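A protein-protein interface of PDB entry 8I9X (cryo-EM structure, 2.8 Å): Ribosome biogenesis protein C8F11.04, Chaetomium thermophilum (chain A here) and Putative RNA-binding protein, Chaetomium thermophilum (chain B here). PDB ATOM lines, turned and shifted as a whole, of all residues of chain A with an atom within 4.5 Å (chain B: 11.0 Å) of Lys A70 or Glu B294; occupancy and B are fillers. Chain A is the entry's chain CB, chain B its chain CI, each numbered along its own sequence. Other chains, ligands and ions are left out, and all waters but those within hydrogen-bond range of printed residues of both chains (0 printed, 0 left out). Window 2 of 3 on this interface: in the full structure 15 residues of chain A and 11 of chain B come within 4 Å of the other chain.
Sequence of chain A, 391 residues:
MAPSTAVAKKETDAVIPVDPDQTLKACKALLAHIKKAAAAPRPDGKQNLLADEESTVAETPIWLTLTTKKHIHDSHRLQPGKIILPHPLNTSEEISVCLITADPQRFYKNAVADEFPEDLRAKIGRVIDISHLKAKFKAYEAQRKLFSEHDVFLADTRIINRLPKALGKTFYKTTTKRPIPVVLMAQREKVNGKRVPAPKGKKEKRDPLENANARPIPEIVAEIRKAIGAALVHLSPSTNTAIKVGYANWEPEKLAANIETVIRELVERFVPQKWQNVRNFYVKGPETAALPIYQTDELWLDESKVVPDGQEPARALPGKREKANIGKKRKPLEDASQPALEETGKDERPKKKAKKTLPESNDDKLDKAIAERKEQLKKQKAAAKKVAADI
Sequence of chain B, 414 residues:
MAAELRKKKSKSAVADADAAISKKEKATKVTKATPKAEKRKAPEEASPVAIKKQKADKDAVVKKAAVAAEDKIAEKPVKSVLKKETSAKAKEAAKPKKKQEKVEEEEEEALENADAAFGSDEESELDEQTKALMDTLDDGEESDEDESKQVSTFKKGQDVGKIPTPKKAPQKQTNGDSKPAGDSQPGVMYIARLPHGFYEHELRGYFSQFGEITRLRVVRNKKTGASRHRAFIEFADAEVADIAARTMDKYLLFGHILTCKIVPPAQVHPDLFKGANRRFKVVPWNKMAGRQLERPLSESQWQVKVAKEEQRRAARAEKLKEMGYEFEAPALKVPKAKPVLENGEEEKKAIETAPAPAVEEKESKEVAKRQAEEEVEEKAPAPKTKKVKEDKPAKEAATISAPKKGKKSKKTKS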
ATOM      1  N   THR A  68     -10.726   0.456  14.460  1.00  0.00           N
ATOM      2  CA  THR A  68      -9.915  -0.119  15.550  1.00  0.00           C
ATOM      3  C   THR A  68     -10.819  -0.888  16.514  1.00  0.00           C
ATOM      4  O   THR A  68     -12.053  -0.840  16.335  1.00  0.00           O
ATOM      5  CB  THR A  68      -9.109   1.001  16.217  1.00  0.00           C
ATOM      6  OG1 THR A  68      -8.792   0.659  17.566  1.00  0.00           O
ATOM      7  CG2 THR A  68      -9.856   2.313  16.208  1.00  0.00           C
ATOM      8  N   LYS A  69     -10.230  -1.588  17.474  1.00  0.00           N
ATOM      9  CA  LYS A  69     -10.962  -2.340  18.485  1.00  0.00           C
ATOM     10  C   LYS A  69     -10.989  -1.647  19.843  1.00  0.00           C
ATOM     11  O   LYS A  69     -11.445  -2.249  20.821  1.00  0.00           O
ATOM     12  CB  LYS A  69     -10.362  -3.739  18.635  1.00  0.00           C
ATOM     13  CG  LYS A  69      -8.937  -3.747  19.163  1.00  0.00           C
ATOM     14  CD  LYS A  69      -8.409  -5.163  19.314  1.00  0.00           C
ATOM     15  CE  LYS A  69      -8.139  -5.804  17.964  1.00  0.00           C
ATOM     16  NZ  LYS A  69      -7.032  -5.119  17.243  1.00  0.00           N
ATOM     17  N   LYS A  70     -10.514  -0.409  19.931  1.00  0.00           N
ATOM     18  CA  LYS A  70     -10.520   0.341  21.179  1.00  0.00           C
ATOM     19  C   LYS A  70     -10.655   1.819  20.846  1.00  0.00           C
ATOM     20  O   LYS A  70     -10.278   2.267  19.761  1.00  0.00           O
ATOM     21  CB  LYS A  70      -9.250   0.063  22.003  1.00  0.00           C
ATOM     22  CG  LYS A  70      -9.161   0.810  23.332  1.00  0.00           C
ATOM     23  CD  LYS A  70      -7.918   0.443  24.131  1.00  0.00           C
ATOM     24  CE  LYS A  70      -6.645   0.677  23.342  1.00  0.00           C
ATOM     25  NZ  LYS A  70      -6.558   2.084  22.862  1.00  0.00           N
ATOM     26  N   HIS A  71     -11.211   2.581  21.784  1.00  0.00           N
ATOM     27  CA  HIS A  71     -11.334   4.018  21.585  1.00  0.00           C
ATOM     28  C   HIS A  71      -9.962   4.650  21.401  1.00  0.00           C
ATOM     29  O   HIS A  71      -9.030   4.385  22.166  1.00  0.00           O
ATOM     30  CB  HIS A  71     -12.051   4.660  22.769  1.00  0.00           C
ATOM     31  CG  HIS A  71     -13.541   4.603  22.672  1.00  0.00           C
ATOM     32  ND1 HIS A  71     -14.251   5.305  21.724  1.00  0.00           N
ATOM     33  CD2 HIS A  71     -14.458   3.935  23.407  1.00  0.00           C
ATOM     34  CE1 HIS A  71     -15.542   5.067  21.875  1.00  0.00           C
ATOM     35  NE2 HIS A  71     -15.694   4.239  22.892  1.00  0.00           N
ATOM     36  N   ILE A  72      -9.842   5.487  20.371  1.00  0.00           N
ATOM     37  CA  ILE A  72      -8.562   6.123  20.081  1.00  0.00           C
ATOM     38  C   ILE A  72      -8.177   7.087  21.193  1.00  0.00           C
ATOM     39  O   ILE A  72      -7.020   7.122  21.630  1.00  0.00           O
ATOM     40  CB  ILE A  72      -8.616   6.824  18.713  1.00  0.00           C
ATOM     41  CG1 ILE A  72      -8.945   5.816  17.613  1.00  0.00           C
ATOM     42  CG2 ILE A  72      -7.294   7.498  18.413  1.00  0.00           C
ATOM     43  CD1 ILE A  72      -7.919   4.714  17.479  1.00  0.00           C
ATOM     44  N   THR A 239     -14.100   4.336  17.438  1.00  0.00           N
ATOM     45  CA  THR A 239     -13.222   3.359  16.800  1.00  0.00           C
ATOM     46  C   THR A 239     -13.167   3.553  15.292  1.00  0.00           C
ATOM     47  O   THR A 239     -13.019   2.590  14.535  1.00  0.00           O
ATOM     48  CB  THR A 239     -13.679   1.946  17.140  1.00  0.00           C
ATOM     49  OG1 THR A 239     -15.082   1.824  16.878  1.00  0.00           O
ATOM     50  CG2 THR A 239     -13.418   1.643  18.607  1.00  0.00           C
ATOM     51  N   PRO A 272      -3.049   4.362  20.386  1.00  0.00           N
ATOM     52  CA  PRO A 272      -2.525   3.597  21.520  1.00  0.00           C
ATOM     53  C   PRO A 272      -2.453   2.113  21.199  1.00  0.00           C
ATOM     54  O   PRO A 272      -3.235   1.587  20.404  1.00  0.00           O
ATOM     55  CB  PRO A 272      -3.540   3.872  22.635  1.00  0.00           C
ATOM     56  CG  PRO A 272      -4.231   5.130  22.226  1.00  0.00           C
ATOM     57  CD  PRO A 272      -4.282   5.085  20.730  1.00  0.00           C
ATOM     58  N   GLN A 273      -1.475   1.446  21.816  1.00  0.00           N
ATOM     59  CA  GLN A 273      -1.274   0.000  21.743  1.00  0.00           C
ATOM     60  C   GLN A 273      -0.824  -0.472  20.363  1.00  0.00           C
ATOM     61  O   GLN A 273      -0.525  -1.658  20.184  1.00  0.00           O
ATOM     62  CB  GLN A 273      -2.532  -0.762  22.173  1.00  0.00           C
ATOM     63  CG  GLN A 273      -2.946  -0.500  23.610  1.00  0.00           C
ATOM     64  CD  GLN A 273      -1.880  -0.909  24.606  1.00  0.00           C
ATOM     65  OE1 GLN A 273      -1.237  -0.063  25.227  1.00  0.00           O
ATOM     66  NE2 GLN A 273      -1.686  -2.214  24.764  1.00  0.00           N
ATOM     67  N   ASN A 277      -3.882  -2.866  18.849  1.00  0.00           N
ATOM     68  CA  ASN A 277      -5.129  -2.132  18.710  1.00  0.00           C
ATOM     69  C   ASN A 277      -5.573  -1.967  17.267  1.00  0.00           C
ATOM     70  O   ASN A 277      -6.774  -1.802  17.024  1.00  0.00           O
ATOM     71  CB  ASN A 277      -4.998  -0.743  19.338  1.00  0.00           C
ATOM     72  CG  ASN A 277      -6.336  -0.136  19.694  1.00  0.00           C
ATOM     73  OD1 ASN A 277      -7.380  -0.770  19.543  1.00  0.00           O
ATOM     74  ND2 ASN A 277      -6.318   1.114  20.135  1.00  0.00           N
ATOM     75  N   TRP B 285     -23.121   7.940  26.828  1.00  0.00           N
ATOM     76  CA  TRP B 285     -23.366   6.783  25.976  1.00  0.00           C
ATOM     77  C   TRP B 285     -22.098   6.326  25.272  1.00  0.00           C
ATOM     78  O   TRP B 285     -21.879   5.121  25.107  1.00  0.00           O
ATOM     79  CB  TRP B 285     -24.459   7.109  24.959  1.00  0.00           C
ATOM     80  CG  TRP B 285     -25.824   7.234  25.563  1.00  0.00           C
ATOM     81  CD1 TRP B 285     -26.552   8.377  25.707  1.00  0.00           C
ATOM     82  CD2 TRP B 285     -26.631   6.177  26.094  1.00  0.00           C
ATOM     83  NE1 TRP B 285     -27.758   8.100  26.301  1.00  0.00           N
ATOM     84  CE2 TRP B 285     -27.833   6.756  26.545  1.00  0.00           C
ATOM     85  CE3 TRP B 285     -26.453   4.797  26.231  1.00  0.00           C
ATOM     86  CZ2 TRP B 285     -28.851   6.004  27.127  1.00  0.00           C
ATOM     87  CZ3 TRP B 285     -27.466   4.052  26.808  1.00  0.00           C
ATOM     88  CH2 TRP B 285     -28.650   4.658  27.249  1.00  0.00           C
ATOM     89  N   ASN B 286     -21.249   7.266  24.850  1.00  0.00           N
ATOM     90  CA  ASN B 286     -19.984   6.891  24.226  1.00  0.00           C
ATOM     91  C   ASN B 286     -19.076   6.146  25.197  1.00  0.00           C
ATOM     92  O   ASN B 286     -18.469   5.132  24.831  1.00  0.00           O
ATOM     93  CB  ASN B 286     -19.283   8.132  23.673  1.00  0.00           C
ATOM     94  CG  ASN B 286     -18.998   9.175  24.741  1.00  0.00           C
ATOM     95  OD1 ASN B 286     -19.229   8.949  25.930  1.00  0.00           O
ATOM     96  ND2 ASN B 286     -18.490  10.326  24.319  1.00  0.00           N
ATOM     97  N   LYS B 287     -18.976   6.628  26.439  1.00  0.00           N
ATOM     98  CA  LYS B 287     -18.146   5.955  27.430  1.00  0.00           C
ATOM     99  C   LYS B 287     -18.689   4.572  27.764  1.00  0.00           C
ATOM    100  O   LYS B 287     -17.912   3.623  27.947  1.00  0.00           O
ATOM    101  CB  LYS B 287     -18.037   6.828  28.682  1.00  0.00           C
ATOM    102  CG  LYS B 287     -17.121   6.290  29.768  1.00  0.00           C
ATOM    103  CD  LYS B 287     -16.931   7.322  30.874  1.00  0.00           C
ATOM    104  CE  LYS B 287     -18.204   7.537  31.677  1.00  0.00           C
ATOM    105  NZ  LYS B 287     -18.007   8.480  32.814  1.00  0.00           N
ATOM    106  N   MET B 288     -20.014   4.434  27.839  1.00  0.00           N
ATOM    107  CA  MET B 288     -20.607   3.118  28.042  1.00  0.00           C
ATOM    108  C   MET B 288     -20.312   2.177  26.887  1.00  0.00           C
ATOM    109  O   MET B 288     -19.930   1.025  27.112  1.00  0.00           O
ATOM    110  CB  MET B 288     -22.114   3.230  28.233  1.00  0.00           C
ATOM    111  CG  MET B 288     -22.509   3.912  29.503  1.00  0.00           C
ATOM    112  SD  MET B 288     -24.291   4.012  29.654  1.00  0.00           S
ATOM    113  CE  MET B 288     -24.378   4.929  31.172  1.00  0.00           C
ATOM    114  N   ALA B 289     -20.500   2.637  25.649  1.00  0.00           N
ATOM    115  CA  ALA B 289     -20.202   1.792  24.501  1.00  0.00           C
ATOM    116  C   ALA B 289     -18.744   1.375  24.488  1.00  0.00           C
ATOM    117  O   ALA B 289     -18.441   0.208  24.209  1.00  0.00           O
ATOM    118  CB  ALA B 289     -20.561   2.516  23.202  1.00  0.00           C
ATOM    119  N   GLY B 290     -17.839   2.288  24.821  1.00  0.00           N
ATOM    120  CA  GLY B 290     -16.447   1.935  24.963  1.00  0.00           C
ATOM    121  C   GLY B 290     -16.227   0.842  25.980  1.00  0.00           C
ATOM    122  O   GLY B 290     -15.899  -0.291  25.611  1.00  0.00           O
ATOM    123  N   ARG B 291     -16.454   1.139  27.258  1.00  0.00           N
ATOM    124  CA  ARG B 291     -16.145   0.133  28.267  1.00  0.00           C
ATOM    125  C   ARG B 291     -16.916  -1.168  28.062  1.00  0.00           C
ATOM    126  O   ARG B 291     -16.406  -2.227  28.441  1.00  0.00           O
ATOM    127  CB  ARG B 291     -16.360   0.716  29.664  1.00  0.00           C
ATOM    128  CG  ARG B 291     -15.347   1.816  29.962  1.00  0.00           C
ATOM    129  CD  ARG B 291     -15.517   2.457  31.325  1.00  0.00           C
ATOM    130  NE  ARG B 291     -16.748   3.228  31.429  1.00  0.00           N
ATOM    131  CZ  ARG B 291     -17.193   3.772  32.552  1.00  0.00           C
ATOM    132  NH1 ARG B 291     -16.555   3.609  33.699  1.00  0.00           N
ATOM    133  NH2 ARG B 291     -18.301   4.505  32.520  1.00  0.00           N
ATOM    134  N   GLN B 292     -18.062  -1.141  27.387  1.00  0.00           N
ATOM    135  CA  GLN B 292     -18.681  -2.361  26.887  1.00  0.00           C
ATOM    136  C   GLN B 292     -17.817  -3.070  25.851  1.00  0.00           C
ATOM    137  O   GLN B 292     -17.740  -4.303  25.866  1.00  0.00           O
ATOM    138  CB  GLN B 292     -20.055  -2.043  26.288  1.00  0.00           C
ATOM    139  CG  GLN B 292     -20.806  -3.247  25.742  1.00  0.00           C
ATOM    140  CD  GLN B 292     -21.105  -4.286  26.803  1.00  0.00           C
ATOM    141  OE1 GLN B 292     -21.539  -3.957  27.906  1.00  0.00           O
ATOM    142  NE2 GLN B 292     -20.885  -5.553  26.470  1.00  0.00           N
ATOM    143  N   LEU B 293     -17.168  -2.322  24.959  1.00  0.00           N
ATOM    144  CA  LEU B 293     -16.267  -2.901  23.973  1.00  0.00           C
ATOM    145  C   LEU B 293     -15.005  -3.494  24.586  1.00  0.00           C
ATOM    146  O   LEU B 293     -14.539  -4.536  24.113  1.00  0.00           O
ATOM    147  CB  LEU B 293     -15.879  -1.853  22.920  1.00  0.00           C
ATOM    148  CG  LEU B 293     -15.018  -2.314  21.743  1.00  0.00           C
ATOM    149  CD1 LEU B 293     -15.791  -3.272  20.853  1.00  0.00           C
ATOM    150  CD2 LEU B 293     -14.523  -1.117  20.947  1.00  0.00           C
ATOM    151  N   GLU B 294     -14.439  -2.870  25.618  1.00  0.00           N
ATOM    152  CA  GLU B 294     -13.275  -3.449  26.292  1.00  0.00           C
ATOM    153  C   GLU B 294     -13.644  -4.419  27.408  1.00  0.00           C
ATOM    154  O   GLU B 294     -12.745  -4.992  28.030  1.00  0.00           O
ATOM    155  CB  GLU B 294     -12.312  -2.395  26.860  1.00  0.00           C
ATOM    156  CG  GLU B 294     -11.570  -1.534  25.843  1.00  0.00           C
ATOM    157  CD  GLU B 294     -12.380  -0.366  25.369  1.00  0.00           C
ATOM    158  OE1 GLU B 294     -13.486  -0.196  25.889  1.00  0.00           O
ATOM    159  OE2 GLU B 294     -11.927   0.379  24.479  1.00  0.00           O
ATOM    160  N   ARG B 295     -14.928  -4.621  27.686  1.00  0.00           N
ATOM    161  CA  ARG B 295     -15.320  -5.648  28.645  1.00  0.00           C
ATOM    162  C   ARG B 295     -15.064  -7.030  28.058  1.00  0.00           C
ATOM    163  O   ARG B 295     -15.621  -7.359  27.000  1.00  0.00           O
ATOM    164  CB  ARG B 295     -16.795  -5.495  29.021  1.00  0.00           C
ATOM    165  CG  ARG B 295     -17.326  -6.596  29.926  1.00  0.00           C
ATOM    166  CD  ARG B 295     -16.680  -6.544  31.301  1.00  0.00           C
ATOM    167  NE  ARG B 295     -17.255  -7.529  32.211  1.00  0.00           N
ATOM    168  CZ  ARG B 295     -16.816  -8.772  32.348  1.00  0.00           C
ATOM    169  NH1 ARG B 295     -15.790  -9.225  31.647  1.00  0.00           N
ATOM    170  NH2 ARG B 295     -17.422  -9.582  33.212  1.00  0.00           N
ATOM    171  N   PRO B 296     -14.242  -7.863  28.694  1.00  0.00           N
ATOM    172  CA  PRO B 296     -13.978  -9.201  28.152  1.00  0.00           C
ATOM    173  C   PRO B 296     -15.205 -10.097  28.230  1.00  0.00           C
ATOM    174  O   PRO B 296     -16.055  -9.964  29.113  1.00  0.00           O
ATOM    175  CB  PRO B 296     -12.849  -9.735  29.042  1.00  0.00           C
ATOM    176  CG  PRO B 296     -12.317  -8.539  29.776  1.00  0.00           C
ATOM    177  CD  PRO B 296     -13.465  -7.601  29.915  1.00  0.00           C
ATOM    178  N   LEU B 297     -15.280 -11.024  27.285  1.00  0.00           N
ATOM    179  CA  LEU B 297     -16.375 -11.991  27.208  1.00  0.00           C
ATOM    180  C   LEU B 297     -15.912 -13.127  26.299  1.00  0.00           C
ATOM    181  O   LEU B 297     -15.032 -12.941  25.450  1.00  0.00           O
ATOM    182  CB  LEU B 297     -17.662 -11.312  26.728  1.00  0.00           C
ATOM    183  CG  LEU B 297     -19.002 -12.056  26.737  1.00  0.00           C
ATOM    184  CD1 LEU B 297     -20.136 -11.058  26.891  1.00  0.00           C
ATOM    185  CD2 LEU B 297     -19.204 -12.858  25.469  1.00  0.00           C
ATOM    186  N   SER B 298     -16.500 -14.311  26.479  1.00  0.00           N
ATOM    187  CA  SER B 298     -16.137 -15.487  25.692  1.00  0.00           C
ATOM    188  C   SER B 298     -16.526 -15.251  24.238  1.00  0.00           C
ATOM    189  O   SER B 298     -17.711 -15.110  23.918  1.00  0.00           O
ATOM    190  CB  SER B 298     -16.817 -16.736  26.243  1.00  0.00           C
ATOM    191  OG  SER B 298     -16.589 -17.850  25.396  1.00  0.00           O
ATOM    192  N   GLU B 299     -15.534 -15.233  23.354  1.00  0.00           N
ATOM    193  CA  GLU B 299     -15.739 -14.858  21.958  1.00  0.00           C
ATOM    194  C   GLU B 299     -16.063 -16.045  21.065  1.00  0.00           C
ATOM    195  O   GLU B 299     -15.762 -16.015  19.875  1.00  0.00           O
ATOM    196  CB  GLU B 299     -14.514 -14.113  21.441  1.00  0.00           C
ATOM    197  CG  GLU B 299     -14.298 -12.756  22.092  1.00  0.00           C
ATOM    198  CD  GLU B 299     -13.064 -12.047  21.572  1.00  0.00           C
ATOM    199  OE1 GLU B 299     -12.305 -12.665  20.797  1.00  0.00           O
ATOM    200  OE2 GLU B 299     -12.856 -10.870  21.934  1.00  0.00           O
ATOM    201  N   TRP B 302     -18.530 -14.553  19.229  1.00  0.00           N
ATOM    202  CA  TRP B 302     -17.875 -13.561  18.389  1.00  0.00           C
ATOM    203  C   TRP B 302     -17.181 -14.215  17.202  1.00  0.00           C
ATOM    204  O   TRP B 302     -17.008 -13.576  16.168  1.00  0.00           O
ATOM    205  CB  TRP B 302     -16.894 -12.729  19.214  1.00  0.00           C
ATOM    206  CG  TRP B 302     -16.397 -11.516  18.495  1.00  0.00           C
ATOM    207  CD1 TRP B 302     -17.018 -10.306  18.415  1.00  0.00           C
ATOM    208  CD2 TRP B 302     -15.163 -11.383  17.779  1.00  0.00           C
ATOM    209  NE1 TRP B 302     -16.258  -9.430  17.679  1.00  0.00           N
ATOM    210  CE2 TRP B 302     -15.113 -10.067  17.279  1.00  0.00           C
ATOM    211  CE3 TRP B 302     -14.099 -12.249  17.507  1.00  0.00           C
ATOM    212  CZ2 TRP B 302     -14.042  -9.595  16.523  1.00  0.00           C
ATOM    213  CZ3 TRP B 302     -13.035 -11.778  16.757  1.00  0.00           C
ATOM    214  CH2 TRP B 302     -13.016 -10.463  16.273  1.00  0.00           C
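The backbone NH (N) of Gly B290 lies close to a ring nitrogen (NE2) of His A71, 3.5 Å away.
The side-chain carboxylate (OE1) of Glu B294 lies close to the backbone carbonyl oxygen (O) of Gly B290 (2.4 Å). OG1 of Thr A68 is in hydrogen-bond range of O of Lys A70, 3.1 Å away. The backbone carbonyl oxygen (O) of Thr A239 sits at hydrogen-bond distance from the backbone NH (N) of Thr A68 (3.1 Å). The backbone carbonyl oxygen of Asn A277 is in hydrogen-bond range of the side-chain amino group of Lys A69 (3.3 Å). NZ of Lys A70 lies close to ND2 of Asn A277 (2.9 Å).
Among the printed residues, merely in contact across the chains: Lys A69 with Leu B293 (3.3 Å), Lys A70 with Glu B294 (3.0 Å), His A71 with Asn B286 (3.5 Å), His A71 with Glu B294 (3.6 Å) and Thr A239 with Leu B293 (3.8 Å).
No residue of chain B comes within 4 Å of Thr A68. Lys A69 touches just one residue of chain B: Leu B293. Of chain B, only Glu B294 (3.0 Å) comes within 4 Å of Lys A70. Of chain B, only Asn B286, Gly B290 and Glu B294 come within 4 Å of His A71. No residue of chain B comes within 4 Å of Ile A72. Thr A239 touches one residue of chain B. No residue of chain B comes within 4 Å of Pro A272. No residue of chain B comes within 4 Å of Asn A277. Of the printed residues of chain A, Asn B286 touches His A71 (3.5 Å). Of the printed residues of chain A, Gly B290 touches His A71 (3.2 Å). Of the printed residues of chain A, Leu B293 touches Lys A69 (3.3 Å) and Thr A239 (3.8 Å). Glu B294 touches just these residues of chain A: Lys A70 (3.0 Å) and His A71 (3.6 Å). Ser B298 touches none of the printed residues of chain A. The nearest residue of chain B that does not touch Lys A70 is Leu B293 (4.2 Å). The nearest printed residue of chain A that does not touch Glu B294 is Lys A69 (4.5 Å). The nearest printed residue of chain A that does not touch Asn B286 is Thr A239 (8.6 Å).
Hydrophobic or aromatic side chains of chain B within 4 Å of the printed part of chain A: Leu B293. Of the 9 printed residues of chain A, 4 touch a printed residue of chain B. Among the printed residues, 6 pairs touch across the chains. Among the printed residues, no Asp or Glu carboxylate lies within 4 Å of a Lys or Arg side-chain nitrogen of the other chain.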
